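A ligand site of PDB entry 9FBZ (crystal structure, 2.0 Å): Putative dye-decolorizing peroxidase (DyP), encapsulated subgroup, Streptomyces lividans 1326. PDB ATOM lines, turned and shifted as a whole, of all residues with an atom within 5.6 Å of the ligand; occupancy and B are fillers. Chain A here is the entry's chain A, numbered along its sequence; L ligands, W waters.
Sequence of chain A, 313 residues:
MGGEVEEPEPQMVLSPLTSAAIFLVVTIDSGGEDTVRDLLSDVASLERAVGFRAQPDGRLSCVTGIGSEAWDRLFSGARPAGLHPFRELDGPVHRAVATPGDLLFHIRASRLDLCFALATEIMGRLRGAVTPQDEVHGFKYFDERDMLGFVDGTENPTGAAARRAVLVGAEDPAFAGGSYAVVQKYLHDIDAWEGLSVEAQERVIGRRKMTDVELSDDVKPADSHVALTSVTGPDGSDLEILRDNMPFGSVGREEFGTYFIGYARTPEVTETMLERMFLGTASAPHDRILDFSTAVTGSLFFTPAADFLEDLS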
ATOM      1  N   ASP A 146       3.931 -23.527  16.011  1.00  0.00           N
ATOM      2  CA  ASP A 146       3.909 -22.639  14.861  1.00  0.00           C
ATOM      3  C   ASP A 146       4.263 -23.476  13.629  1.00  0.00           C
ATOM      4  O   ASP A 146       4.430 -24.702  13.740  1.00  0.00           O
ATOM      5  CB  ASP A 146       4.783 -21.401  15.082  1.00  0.00           C
ATOM      6  CG  ASP A 146       6.228 -21.642  15.391  1.00  0.00           C
ATOM      7  OD1 ASP A 146       6.755 -22.698  14.863  1.00  0.00           O
ATOM      8  OD2 ASP A 146       6.828 -20.778  16.120  1.00  0.00           O
ATOM      9  N   LEU A 148       6.977 -23.679  12.030  1.00  0.00           N
ATOM     10  CA  LEU A 148       8.296 -24.319  12.127  1.00  0.00           C
ATOM     11  C   LEU A 148       8.287 -25.588  12.984  1.00  0.00           C
ATOM     12  O   LEU A 148       9.279 -26.320  13.005  1.00  0.00           O
ATOM     13  CB  LEU A 148       9.315 -23.318  12.654  1.00  0.00           C
ATOM     14  CG  LEU A 148       9.452 -22.021  11.845  1.00  0.00           C
ATOM     15  CD1 LEU A 148      10.424 -21.066  12.501  1.00  0.00           C
ATOM     16  CD2 LEU A 148       9.829 -22.322  10.414  1.00  0.00           C
ATOM     17  N   PHE A 150       7.759 -25.715  16.290  1.00  0.00           N
ATOM     18  CA  PHE A 150       8.112 -25.403  17.689  1.00  0.00           C
ATOM     19  C   PHE A 150       6.912 -24.783  18.419  1.00  0.00           C
ATOM     20  O   PHE A 150       6.116 -24.029  17.845  1.00  0.00           O
ATOM     21  CB  PHE A 150       9.322 -24.465  17.732  1.00  0.00           C
ATOM     22  CG  PHE A 150      10.636 -25.144  17.463  1.00  0.00           C
ATOM     23  CD1 PHE A 150      10.943 -25.646  16.200  1.00  0.00           C
ATOM     24  CD2 PHE A 150      11.517 -25.408  18.497  1.00  0.00           C
ATOM     25  CE1 PHE A 150      12.121 -26.350  15.960  1.00  0.00           C
ATOM     26  CE2 PHE A 150      12.695 -26.080  18.251  1.00  0.00           C
ATOM     27  CZ  PHE A 150      13.005 -26.552  16.995  1.00  0.00           C
ATOM     28  N   VAL A 151       6.809 -25.088  19.725  1.00  0.00           N
ATOM     29  CA  VAL A 151       5.819 -24.478  20.601  1.00  0.00           C
ATOM     30  C   VAL A 151       6.128 -22.996  20.653  1.00  0.00           C
ATOM     31  O   VAL A 151       7.290 -22.588  20.768  1.00  0.00           O
ATOM     32  CB  VAL A 151       5.817 -25.107  22.010  1.00  0.00           C
ATOM     33  CG1 VAL A 151       4.803 -24.495  22.931  1.00  0.00           C
ATOM     34  CG2 VAL A 151       5.571 -26.618  21.971  1.00  0.00           C
ATOM     35  N   ASP A 152       5.049 -22.196  20.553  1.00  0.00           N
ATOM     36  CA  ASP A 152       5.186 -20.749  20.369  1.00  0.00           C
ATOM     37  C   ASP A 152       4.338 -20.034  21.432  1.00  0.00           C
ATOM     38  O   ASP A 152       3.109 -20.182  21.407  1.00  0.00           O
ATOM     39  CB  ASP A 152       4.760 -20.418  18.930  1.00  0.00           C
ATOM     40  CG  ASP A 152       5.161 -19.041  18.468  1.00  0.00           C
ATOM     41  OD1 ASP A 152       5.034 -18.113  19.301  1.00  0.00           O
ATOM     42  OD2 ASP A 152       5.629 -18.907  17.276  1.00  0.00           O
ATOM     43  N   GLY A 153       4.989 -19.276  22.331  1.00  0.00           N
ATOM     44  CA  GLY A 153       4.300 -18.497  23.378  1.00  0.00           C
ATOM     45  C   GLY A 153       4.707 -18.866  24.826  1.00  0.00           C
ATOM     46  O   GLY A 153       4.364 -18.161  25.753  1.00  0.00           O
ATOM     47  N   THR A 154       5.539 -19.899  25.004  1.00  0.00           N
ATOM     48  CA  THR A 154       5.835 -20.463  26.299  1.00  0.00           C
ATOM     49  C   THR A 154       6.321 -19.449  27.326  1.00  0.00           C
ATOM     50  O   THR A 154       5.859 -19.460  28.452  1.00  0.00           O
ATOM     51  CB  THR A 154       6.904 -21.546  26.143  1.00  0.00           C
ATOM     52  OG1 THR A 154       6.494 -22.403  25.085  1.00  0.00           O
ATOM     53  CG2 THR A 154       7.032 -22.347  27.425  1.00  0.00           C
ATOM     54  N   GLU A 155       7.286 -18.582  26.961  1.00  0.00           N
ATOM     55  CA  GLU A 155       7.876 -17.632  27.883  1.00  0.00           C
ATOM     56  C   GLU A 155       7.157 -16.278  27.892  1.00  0.00           C
ATOM     57  O   GLU A 155       7.699 -15.301  28.425  1.00  0.00           O
ATOM     58  CB  GLU A 155       9.373 -17.441  27.592  1.00  0.00           C
ATOM     59  CG  GLU A 155      10.238 -18.622  28.008  1.00  0.00           C
ATOM     60  CD  GLU A 155      10.155 -18.972  29.462  1.00  0.00           C
ATOM     61  OE1 GLU A 155      10.588 -18.104  30.206  1.00  0.00           O
ATOM     62  OE2 GLU A 155       9.641 -20.051  29.824  1.00  0.00           O
ATOM     63  N   ASN A 156       5.937 -16.174  27.343  1.00  0.00           N
ATOM     64  CA  ASN A 156       5.195 -14.938  27.553  1.00  0.00           C
ATOM     65  C   ASN A 156       5.044 -14.675  29.065  1.00  0.00           C
ATOM     66  O   ASN A 156       4.803 -15.582  29.849  1.00  0.00           O
ATOM     67  CB  ASN A 156       3.810 -14.964  26.944  1.00  0.00           C
ATOM     68  CG  ASN A 156       3.753 -14.514  25.508  1.00  0.00           C
ATOM     69  OD1 ASN A 156       4.482 -13.631  25.096  1.00  0.00           O
ATOM     70  ND2 ASN A 156       2.919 -15.157  24.713  1.00  0.00           N
ATOM     71  N   GLN A 184       4.349  -7.843  12.190  1.00  0.00           N
ATOM     72  CA  GLN A 184       5.070  -8.232  10.999  1.00  0.00           C
ATOM     73  C   GLN A 184       4.528  -9.568  10.489  1.00  0.00           C
ATOM     74  O   GLN A 184       4.437 -10.549  11.227  1.00  0.00           O
ATOM     75  CB  GLN A 184       6.551  -8.412  11.307  1.00  0.00           C
ATOM     76  CG  GLN A 184       7.311  -7.192  11.850  1.00  0.00           C
ATOM     77  CD  GLN A 184       8.740  -7.637  12.098  1.00  0.00           C
ATOM     78  OE1 GLN A 184       9.035  -8.453  13.007  1.00  0.00           O
ATOM     79  NE2 GLN A 184       9.629  -7.169  11.235  1.00  0.00           N
ATOM     80  N   TYR A 186       5.338 -12.773   8.509  1.00  0.00           N
ATOM     81  CA  TYR A 186       6.493 -13.549   8.036  1.00  0.00           C
ATOM     82  C   TYR A 186       6.025 -14.711   7.168  1.00  0.00           C
ATOM     83  O   TYR A 186       5.015 -15.363   7.498  1.00  0.00           O
ATOM     84  CB  TYR A 186       7.304 -14.116   9.202  1.00  0.00           C
ATOM     85  CG  TYR A 186       8.182 -13.132   9.959  1.00  0.00           C
ATOM     86  CD1 TYR A 186       9.492 -12.878   9.561  1.00  0.00           C
ATOM     87  CD2 TYR A 186       7.705 -12.455  11.088  1.00  0.00           C
ATOM     88  CE1 TYR A 186      10.272 -11.940  10.233  1.00  0.00           C
ATOM     89  CE2 TYR A 186       8.487 -11.530  11.755  1.00  0.00           C
ATOM     90  CZ  TYR A 186       9.785 -11.280  11.337  1.00  0.00           C
ATOM     91  OH  TYR A 186      10.579 -10.370  11.989  1.00  0.00           O
ATOM     92  N   HIS A 188       7.703 -18.297   5.581  1.00  0.00           N
ATOM     93  CA  HIS A 188       8.796 -19.200   5.884  1.00  0.00           C
ATOM     94  C   HIS A 188       9.154 -19.990   4.627  1.00  0.00           C
ATOM     95  O   HIS A 188       8.268 -20.368   3.895  1.00  0.00           O
ATOM     96  CB  HIS A 188       8.456 -20.168   7.010  1.00  0.00           C
ATOM     97  CG  HIS A 188       8.165 -19.475   8.306  1.00  0.00           C
ATOM     98  ND1 HIS A 188       9.160 -18.811   8.982  1.00  0.00           N
ATOM     99  CD2 HIS A 188       7.020 -19.412   9.050  1.00  0.00           C
ATOM    100  CE1 HIS A 188       8.586 -18.269  10.062  1.00  0.00           C
ATOM    101  NE2 HIS A 188       7.310 -18.653  10.166  1.00  0.00           N
ATOM    102  N   ILE A 205      16.521 -22.094  17.181  1.00  0.00           N
ATOM    103  CA  ILE A 205      15.496 -21.541  18.066  1.00  0.00           C
ATOM    104  C   ILE A 205      16.079 -21.293  19.471  1.00  0.00           C
ATOM    105  O   ILE A 205      15.863 -20.233  20.031  1.00  0.00           O
ATOM    106  CB  ILE A 205      14.281 -22.507  18.130  1.00  0.00           C
ATOM    107  CG1 ILE A 205      13.636 -22.740  16.754  1.00  0.00           C
ATOM    108  CG2 ILE A 205      13.256 -22.037  19.173  1.00  0.00           C
ATOM    109  CD1 ILE A 205      13.056 -21.511  16.132  1.00  0.00           C
ATOM    110  N   ARG A 207      15.633 -23.970  21.957  1.00  0.00           N
ATOM    111  CA  ARG A 207      14.799 -24.836  22.795  1.00  0.00           C
ATOM    112  C   ARG A 207      14.704 -26.194  22.100  1.00  0.00           C
ATOM    113  O   ARG A 207      14.868 -26.271  20.885  1.00  0.00           O
ATOM    114  CB  ARG A 207      13.374 -24.295  22.995  1.00  0.00           C
ATOM    115  CG  ARG A 207      13.302 -22.832  23.469  1.00  0.00           C
ATOM    116  CD  ARG A 207      11.912 -22.309  23.768  1.00  0.00           C
ATOM    117  NE  ARG A 207      11.273 -22.942  24.929  1.00  0.00           N
ATOM    118  CZ  ARG A 207      11.428 -22.505  26.188  1.00  0.00           C
ATOM    119  NH1 ARG A 207      11.954 -21.333  26.424  1.00  0.00           N
ATOM    120  NH2 ARG A 207      10.908 -23.180  27.185  1.00  0.00           N
ATOM    121  N   ASP A 212      10.107 -28.740  24.441  1.00  0.00           N
ATOM    122  CA  ASP A 212      10.056 -27.299  24.653  1.00  0.00           C
ATOM    123  C   ASP A 212      10.846 -26.910  25.906  1.00  0.00           C
ATOM    124  O   ASP A 212      10.580 -25.872  26.503  1.00  0.00           O
ATOM    125  CB  ASP A 212       8.616 -26.818  24.795  1.00  0.00           C
ATOM    126  CG  ASP A 212       8.405 -25.331  24.669  1.00  0.00           C
ATOM    127  OD1 ASP A 212       9.303 -24.622  24.051  1.00  0.00           O
ATOM    128  OD2 ASP A 212       7.336 -24.902  25.191  1.00  0.00           O
ATOM    129  N   GLU A 214      14.158 -25.280  27.391  1.00  0.00           N
ATOM    130  CA  GLU A 214      15.222 -24.395  26.966  1.00  0.00           C
ATOM    131  C   GLU A 214      16.591 -25.118  26.981  1.00  0.00           C
ATOM    132  O   GLU A 214      16.830 -25.871  27.914  1.00  0.00           O
ATOM    133  CB  GLU A 214      15.247 -23.177  27.922  1.00  0.00           C
ATOM    134  CG  GLU A 214      16.167 -22.062  27.470  1.00  0.00           C
ATOM    135  CD  GLU A 214      15.982 -20.756  28.225  1.00  0.00           C
ATOM    136  OE1 GLU A 214      15.092 -20.699  29.089  1.00  0.00           O
ATOM    137  OE2 GLU A 214      16.728 -19.839  27.954  1.00  0.00           O
ATOM    138  N   HIS A 225      17.436 -17.705  18.371  1.00  0.00           N
ATOM    139  CA  HIS A 225      16.314 -16.786  18.504  1.00  0.00           C
ATOM    140  C   HIS A 225      16.097 -16.393  19.970  1.00  0.00           C
ATOM    141  O   HIS A 225      15.914 -15.199  20.286  1.00  0.00           O
ATOM    142  CB  HIS A 225      15.047 -17.402  17.913  1.00  0.00           C
ATOM    143  CG  HIS A 225      13.881 -16.509  17.937  1.00  0.00           C
ATOM    144  ND1 HIS A 225      13.897 -15.265  17.366  1.00  0.00           N
ATOM    145  CD2 HIS A 225      12.655 -16.711  18.418  1.00  0.00           C
ATOM    146  CE1 HIS A 225      12.707 -14.695  17.565  1.00  0.00           C
ATOM    147  NE2 HIS A 225      11.914 -15.559  18.173  1.00  0.00           N
ATOM    148  N   VAL A 226      16.150 -17.371  20.861  1.00  0.00           N
ATOM    149  CA  VAL A 226      15.948 -17.113  22.264  1.00  0.00           C
ATOM    150  C   VAL A 226      17.076 -16.230  22.851  1.00  0.00           C
ATOM    151  O   VAL A 226      16.844 -15.401  23.708  1.00  0.00           O
ATOM    152  CB  VAL A 226      15.757 -18.415  23.055  1.00  0.00           C
ATOM    153  CG1 VAL A 226      15.881 -18.200  24.549  1.00  0.00           C
ATOM    154  CG2 VAL A 226      14.400 -19.046  22.749  1.00  0.00           C
ATOM    155  N   THR A 229      16.584 -12.500  21.681  1.00  0.00           N
ATOM    156  CA  THR A 229      15.377 -11.823  22.119  1.00  0.00           C
ATOM    157  C   THR A 229      15.252 -11.799  23.634  1.00  0.00           C
ATOM    158  O   THR A 229      14.208 -11.386  24.152  1.00  0.00           O
ATOM    159  CB  THR A 229      14.129 -12.424  21.429  1.00  0.00           C
ATOM    160  OG1 THR A 229      14.003 -13.816  21.754  1.00  0.00           O
ATOM    161  CG2 THR A 229      14.193 -12.261  19.928  1.00  0.00           C
ATOM    162  N   SER A 230      16.298 -12.277  24.323  1.00  0.00           N
ATOM    163  CA  SER A 230      16.458 -12.108  25.773  1.00  0.00           C
ATOM    164  C   SER A 230      17.220 -10.818  26.039  1.00  0.00           C
ATOM    165  O   SER A 230      18.399 -10.731  25.644  1.00  0.00           O
ATOM    166  CB  SER A 230      17.177 -13.278  26.381  1.00  0.00           C
ATOM    167  OG  SER A 230      16.436 -14.460  26.170  1.00  0.00           O
ATOM    168  N   ILE A 241       8.011  -8.645  26.431  1.00  0.00           N
ATOM    169  CA  ILE A 241       6.837  -8.305  25.639  1.00  0.00           C
ATOM    170  C   ILE A 241       5.860  -9.460  25.671  1.00  0.00           C
ATOM    171  O   ILE A 241       6.223 -10.556  26.069  1.00  0.00           O
ATOM    172  CB  ILE A 241       7.196  -7.952  24.196  1.00  0.00           C
ATOM    173  CG1 ILE A 241       7.640  -9.167  23.381  1.00  0.00           C
ATOM    174  CG2 ILE A 241       8.236  -6.821  24.185  1.00  0.00           C
ATOM    175  CD1 ILE A 241       7.884  -8.869  21.915  1.00  0.00           C
ATOM    176  N   ARG A 243       3.371 -11.644  23.287  1.00  0.00           N
ATOM    177  CA  ARG A 243       3.200 -12.068  21.906  1.00  0.00           C
ATOM    178  C   ARG A 243       1.962 -12.939  21.760  1.00  0.00           C
ATOM    179  O   ARG A 243       1.582 -13.658  22.708  1.00  0.00           O
ATOM    180  CB  ARG A 243       4.403 -12.890  21.446  1.00  0.00           C
ATOM    181  CG  ARG A 243       5.714 -12.119  21.439  1.00  0.00           C
ATOM    182  CD  ARG A 243       6.879 -13.013  21.234  1.00  0.00           C
ATOM    183  NE  ARG A 243       7.142 -13.772  22.454  1.00  0.00           N
ATOM    184  CZ  ARG A 243       7.146 -15.104  22.549  1.00  0.00           C
ATOM    185  NH1 ARG A 243       7.018 -15.859  21.460  1.00  0.00           N
ATOM    186  NH2 ARG A 243       7.290 -15.683  23.744  1.00  0.00           N
ATOM    187  N   ASN A 245       1.494 -14.781  18.450  1.00  0.00           N
ATOM    188  CA  ASN A 245       1.786 -15.217  17.096  1.00  0.00           C
ATOM    189  C   ASN A 245       0.788 -16.254  16.576  1.00  0.00           C
ATOM    190  O   ASN A 245       0.409 -17.168  17.288  1.00  0.00           O
ATOM    191  CB  ASN A 245       3.177 -15.814  16.972  1.00  0.00           C
ATOM    192  CG  ASN A 245       4.290 -14.861  17.363  1.00  0.00           C
ATOM    193  OD1 ASN A 245       4.091 -13.657  17.549  1.00  0.00           O
ATOM    194  ND2 ASN A 245       5.474 -15.390  17.586  1.00  0.00           N
ATOM    195  N   THR A 258       3.959 -17.135   9.676  1.00  0.00           N
ATOM    196  CA  THR A 258       3.705 -16.738  11.062  1.00  0.00           C
ATOM    197  C   THR A 258       3.349 -15.250  11.066  1.00  0.00           C
ATOM    198  O   THR A 258       4.126 -14.427  10.594  1.00  0.00           O
ATOM    199  CB  THR A 258       4.921 -16.941  11.949  1.00  0.00           C
ATOM    200  OG1 THR A 258       5.323 -18.295  11.940  1.00  0.00           O
ATOM    201  CG2 THR A 258       4.739 -16.473  13.374  1.00  0.00           C
ATOM    202  N   PHE A 260       3.320 -12.259  13.339  1.00  0.00           N
ATOM    203  CA  PHE A 260       3.886 -11.789  14.590  1.00  0.00           C
ATOM    204  C   PHE A 260       3.128 -10.552  15.061  1.00  0.00           C
ATOM    205  O   PHE A 260       2.915  -9.615  14.323  1.00  0.00           O
ATOM    206  CB  PHE A 260       5.388 -11.425  14.421  1.00  0.00           C
ATOM    207  CG  PHE A 260       5.967 -10.710  15.606  1.00  0.00           C
ATOM    208  CD1 PHE A 260       6.359 -11.381  16.741  1.00  0.00           C
ATOM    209  CD2 PHE A 260       6.027  -9.340  15.626  1.00  0.00           C
ATOM    210  CE1 PHE A 260       6.803 -10.681  17.860  1.00  0.00           C
ATOM    211  CE2 PHE A 260       6.515  -8.655  16.729  1.00  0.00           C
ATOM    212  CZ  PHE A 260       6.912  -9.330  17.831  1.00  0.00           C
ATOM    213  N   THR A 270      10.458  -3.534  22.115  1.00  0.00           N
ATOM    214  CA  THR A 270      10.281  -4.289  20.880  1.00  0.00           C
ATOM    215  C   THR A 270      11.338  -3.964  19.850  1.00  0.00           C
ATOM    216  O   THR A 270      11.833  -4.871  19.152  1.00  0.00           O
ATOM    217  CB  THR A 270       8.863  -4.055  20.313  1.00  0.00           C
ATOM    218  OG1 THR A 270       7.900  -4.227  21.338  1.00  0.00           O
ATOM    219  CG2 THR A 270       8.515  -5.085  19.268  1.00  0.00           C
ATOM    220  N   MET A 273      14.751  -5.525  20.554  1.00  0.00           N
ATOM    221  CA  MET A 273      14.752  -6.929  20.131  1.00  0.00           C
ATOM    222  C   MET A 273      14.920  -7.034  18.612  1.00  0.00           C
ATOM    223  O   MET A 273      15.729  -7.834  18.118  1.00  0.00           O
ATOM    224  CB  MET A 273      13.465  -7.627  20.552  1.00  0.00           C
ATOM    225  CG  MET A 273      13.319  -7.795  22.058  1.00  0.00           C
ATOM    226  SD  MET A 273      11.743  -8.449  22.523  1.00  0.00           S
ATOM    227  CE  MET A 273      11.987  -8.636  24.276  1.00  0.00           C
ATOM    228  N   LEU A 274      14.151  -6.241  17.845  1.00  0.00           N
ATOM    229  CA  LEU A 274      14.249  -6.244  16.388  1.00  0.00           C
ATOM    230  C   LEU A 274      15.631  -5.854  15.902  1.00  0.00           C
ATOM    231  O   LEU A 274      16.117  -6.416  14.938  1.00  0.00           O
ATOM    232  CB  LEU A 274      13.204  -5.305  15.779  1.00  0.00           C
ATOM    233  CG  LEU A 274      11.759  -5.793  15.786  1.00  0.00           C
ATOM    234  CD1 LEU A 274      10.827  -4.705  15.378  1.00  0.00           C
ATOM    235  CD2 LEU A 274      11.583  -6.970  14.813  1.00  0.00           C
ATOM    236  N   MET A 277      17.893  -8.792  16.276  1.00  0.00           N
ATOM    237  CA  MET A 277      17.598  -9.817  15.293  1.00  0.00           C
ATOM    238  C   MET A 277      18.151  -9.478  13.908  1.00  0.00           C
ATOM    239  O   MET A 277      18.679 -10.366  13.245  1.00  0.00           O
ATOM    240  CB  MET A 277      16.064 -10.033  15.178  1.00  0.00           C
ATOM    241  CG  MET A 277      15.440 -10.708  16.407  1.00  0.00           C
ATOM    242  SD  MET A 277      13.661 -10.821  16.324  1.00  0.00           S
ATOM    243  CE  MET A 277      13.447 -11.741  14.805  1.00  0.00           C
ATOM    244  N   ILE A 289      16.800 -17.471  12.897  1.00  0.00           N
ATOM    245  CA  ILE A 289      15.433 -17.692  12.427  1.00  0.00           C
ATOM    246  C   ILE A 289      15.176 -16.940  11.119  1.00  0.00           C
ATOM    247  O   ILE A 289      14.367 -17.376  10.313  1.00  0.00           O
ATOM    248  CB  ILE A 289      14.389 -17.376  13.531  1.00  0.00           C
ATOM    249  CG1 ILE A 289      13.138 -18.237  13.392  1.00  0.00           C
ATOM    250  CG2 ILE A 289      13.997 -15.906  13.546  1.00  0.00           C
ATOM    251  CD1 ILE A 289      12.135 -18.072  14.542  1.00  0.00           C
ATOM    252  N   LEU A 290      15.909 -15.846  10.877  1.00  0.00           N
ATOM    253  CA  LEU A 290      15.647 -15.040   9.677  1.00  0.00           C
ATOM    254  C   LEU A 290      16.227 -15.659   8.400  1.00  0.00           C
ATOM    255  O   LEU A 290      15.847 -15.254   7.318  1.00  0.00           O
ATOM    256  CB  LEU A 290      16.200 -13.623   9.859  1.00  0.00           C
ATOM    257  CG  LEU A 290      15.541 -12.831  10.977  1.00  0.00           C
ATOM    258  CD1 LEU A 290      16.279 -11.511  11.159  1.00  0.00           C
ATOM    259  CD2 LEU A 290      14.061 -12.567  10.692  1.00  0.00           C
ATOM    260  N   SER A 293      12.899 -17.194   7.309  1.00  0.00           N
ATOM    261  CA  SER A 293      11.743 -16.350   7.597  1.00  0.00           C
ATOM    262  C   SER A 293      11.978 -14.969   6.990  1.00  0.00           C
ATOM    263  O   SER A 293      12.951 -14.293   7.342  1.00  0.00           O
ATOM    264  CB  SER A 293      11.492 -16.226   9.097  1.00  0.00           C
ATOM    265  OG  SER A 293      11.524 -17.494   9.724  1.00  0.00           O
HETATM  266  C1  LIG L   1      10.391 -16.837  21.646  1.00  0.00           C
HETATM  267  C2  LIG L   1       9.021 -18.161  17.234  1.00  0.00           C
HETATM  268  C3  LIG L   1       9.432 -13.568  15.646  1.00  0.00           C
HETATM  269  C4  LIG L   1      10.362 -12.262  20.162  1.00  0.00           C
HETATM  270  C5  LIG L   1       9.963 -17.570  20.567  1.00  0.00           C
HETATM  271  C6  LIG L   1       9.837 -19.014  20.590  1.00  0.00           C
HETATM  272  C7  LIG L   1       9.463 -19.374  19.342  1.00  0.00           C
HETATM  273  C8  LIG L   1       9.355 -18.212  18.546  1.00  0.00           C
HETATM  274  C9  LIG L   1       9.239 -20.735  18.800  1.00  0.00           C
HETATM  275  C10 LIG L   1      10.174 -19.873  21.771  1.00  0.00           C
HETATM  276  C11 LIG L   1       8.904 -20.188  22.634  1.00  0.00           C
HETATM  277  C12 LIG L   1       8.390 -18.961  23.318  1.00  0.00           C
HETATM  278  O1  LIG L   1       7.581 -18.360  22.668  1.00  0.00           O
HETATM  279  O2  LIG L   1       8.821 -18.535  24.403  1.00  0.00           O
HETATM  280  C13 LIG L   1       9.028 -17.017  16.456  1.00  0.00           C
HETATM  281  C14 LIG L   1       8.762 -17.054  15.040  1.00  0.00           C
HETATM  282  C15 LIG L   1       8.832 -15.799  14.541  1.00  0.00           C
HETATM  283  C16 LIG L   1       9.229 -14.936  15.710  1.00  0.00           C
HETATM  284  C17 LIG L   1       8.323 -18.263  14.197  1.00  0.00           C
HETATM  285  C18 LIG L   1       8.698 -15.580  13.086  1.00  0.00           C
HETATM  286  C19 LIG L   1       9.604 -14.880  12.493  1.00  0.00           C
HETATM  287  C20 LIG L   1       9.744 -12.761  16.723  1.00  0.00           C
HETATM  288  C21 LIG L   1       9.953 -11.326  16.736  1.00  0.00           C
HETATM  289  C22 LIG L   1      10.230 -11.003  18.030  1.00  0.00           C
HETATM  290  C23 LIG L   1      10.207 -12.207  18.796  1.00  0.00           C
HETATM  291  C24 LIG L   1       9.847 -10.402  15.534  1.00  0.00           C
HETATM  292  C25 LIG L   1      10.498  -9.768  18.729  1.00  0.00           C
HETATM  293  C26 LIG L   1      10.595  -8.613  18.226  1.00  0.00           C
HETATM  294  C27 LIG L   1      10.405 -13.442  20.924  1.00  0.00           C
HETATM  295  C28 LIG L   1      10.611 -13.441  22.361  1.00  0.00           C
HETATM  296  C29 LIG L   1      10.694 -14.690  22.783  1.00  0.00           C
HETATM  297  C30 LIG L   1      10.515 -15.464  21.559  1.00  0.00           C
HETATM  298  C31 LIG L   1      10.797 -12.252  23.236  1.00  0.00           C
HETATM  299  C32 LIG L   1      10.884 -15.200  24.213  1.00  0.00           C
HETATM  300  C33 LIG L   1      12.374 -15.256  24.590  1.00  0.00           C
HETATM  301  C34 LIG L   1      12.651 -15.657  26.026  1.00  0.00           C
HETATM  302  O3  LIG L   1      12.688 -14.785  26.861  1.00  0.00           O
HETATM  303  O4  LIG L   1      12.728 -16.829  26.418  1.00  0.00           O
HETATM  304  N1  LIG L   1       9.724 -17.111  19.303  1.00  0.00           N
HETATM  305  N2  LIG L   1       9.297 -15.783  16.769  1.00  0.00           N
HETATM  306  N3  LIG L   1       9.887 -13.233  17.963  1.00  0.00           N
HETATM  307  N4  LIG L   1      10.294 -14.678  20.493  1.00  0.00           N
HETATM  308 FE1  LIG L   1       9.826 -15.197  18.674  1.00  0.00          FE
HETATM  309  O   HOH W   1      12.512 -12.215  26.250  1.00  0.00           O
HETATM  310  O   HOH W   2      11.584 -18.974  24.853  1.00  0.00           O
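NE2 of His 225 binds FE1 of the ligand, at 2.2 Å. N of Gly 153 sits at hydrogen-bond distance from O1 of the ligand. An oxygen (O1) of the ligand lies within salt-bridge range of the guanidinium group (NH1) of Arg 243 (2.8 Å). The backbone NH (N) of Glu 155 lies within hydrogen-bond range of an oxygen (O2) of the ligand. The backbone NH (N) of Thr 154 sits close to an oxygen (O1) of the ligand, 3.5 Å away.
Water W1 bridges an oxygen (O3) of the ligand (2.6 Å) and the backbone carbonyl oxygen (O) of Thr 229 (2.8 Å). Water W2 lies within hydrogen-bond range of an oxygen (O2) of the ligand and the guanidinium group of Arg 207.
The backbone carbonyl oxygen (O) of Ile 205 lies within hydrogen-bond range of the backbone NH (N) of His 225 (3.4 Å). NH1 of Arg 243 lies within salt-bridge range of OD1 of Asp 152 (3.7 Å). The backbone carbonyl oxygen (O) of Arg 243 is in hydrogen-bond range of the side-chain amide nitrogen (ND2) of Asn 156. The side-chain amide oxygen (OE1) of Gln 184 is in hydrogen-bond range of the side-chain hydroxyl (OH) of Tyr 186. ND2 of Asn 245 sits at hydrogen-bond distance from OD1 of Asp 152, 3.2 Å away. OD1 of Asp 146 is in hydrogen-bond range of N of Phe 150. OD1 of Asp 146 sits at hydrogen-bond distance from N of Leu 148, 3.0 Å away. The side-chain carboxylate (OD1) of Asp 212 is in salt-bridge range of the guanidinium group (NE) of Arg 207 (2.7 Å).
OD2 of Asp 146 touches C17 of the ligand, at 3.5 Å. CD1 of Leu 148 touches C17 of the ligand, at 3.9 Å. Phe 150 touches the ligand (CB to C9, 3.9 Å). O of Val 151 touches C9 of the ligand, 3.3 Å away. OD2 of Asp 152 touches C2 of the ligand, 3.5 Å away. OE1 of Gln 184 touches C24 of the ligand (3.3 Å). Tyr 186 touches the ligand (CD2 to C19, 3.4 Å). CD of Arg 207 touches C10 of the ligand, 3.6 Å away. Val 226 touches the ligand (CG1 to O4, 3.9 Å). OG1 of Thr 229 touches C28 of the ligand, 3.5 Å away. OG of Ser 230 touches O3 of the ligand, 3.8 Å away. ND2 of Asn 245 touches N2 of the ligand, 3.9 Å away. OG1 of Thr 258 touches C17 of the ligand, at 3.8 Å. CE1 of Phe 260 touches C21 of the ligand, at 3.4 Å. Met 273 touches the ligand. Leu 274 touches the ligand (CG to C26, 3.9 Å). SD of Met 277 touches C21 of the ligand (3.8 Å). Ile 289 touches the ligand (CD1 to C14, 3.6 Å). Hydrophobic or aromatic side chains within 4 Å of the ligand: Leu 148, Phe 150, Tyr 186, His 225, Val 226, Phe 260, Met 273, Leu 274, Met 277 and Ile 289. Within 4 Å of the ligand: Asp 146, Leu 148, Phe 150, Val 151, Asp 152, Gly 153, Thr 154, Glu 155, Gln 184, Tyr 186, Arg 207, His 225, Val 226, Thr 229, Ser 230, Arg 243, Asn 245, Thr 258, Phe 260, Met 273, Leu 274, Met 277 and Ile 289. The nearest printed residue that does not touch the ligand is His 188 (4.05 Å).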
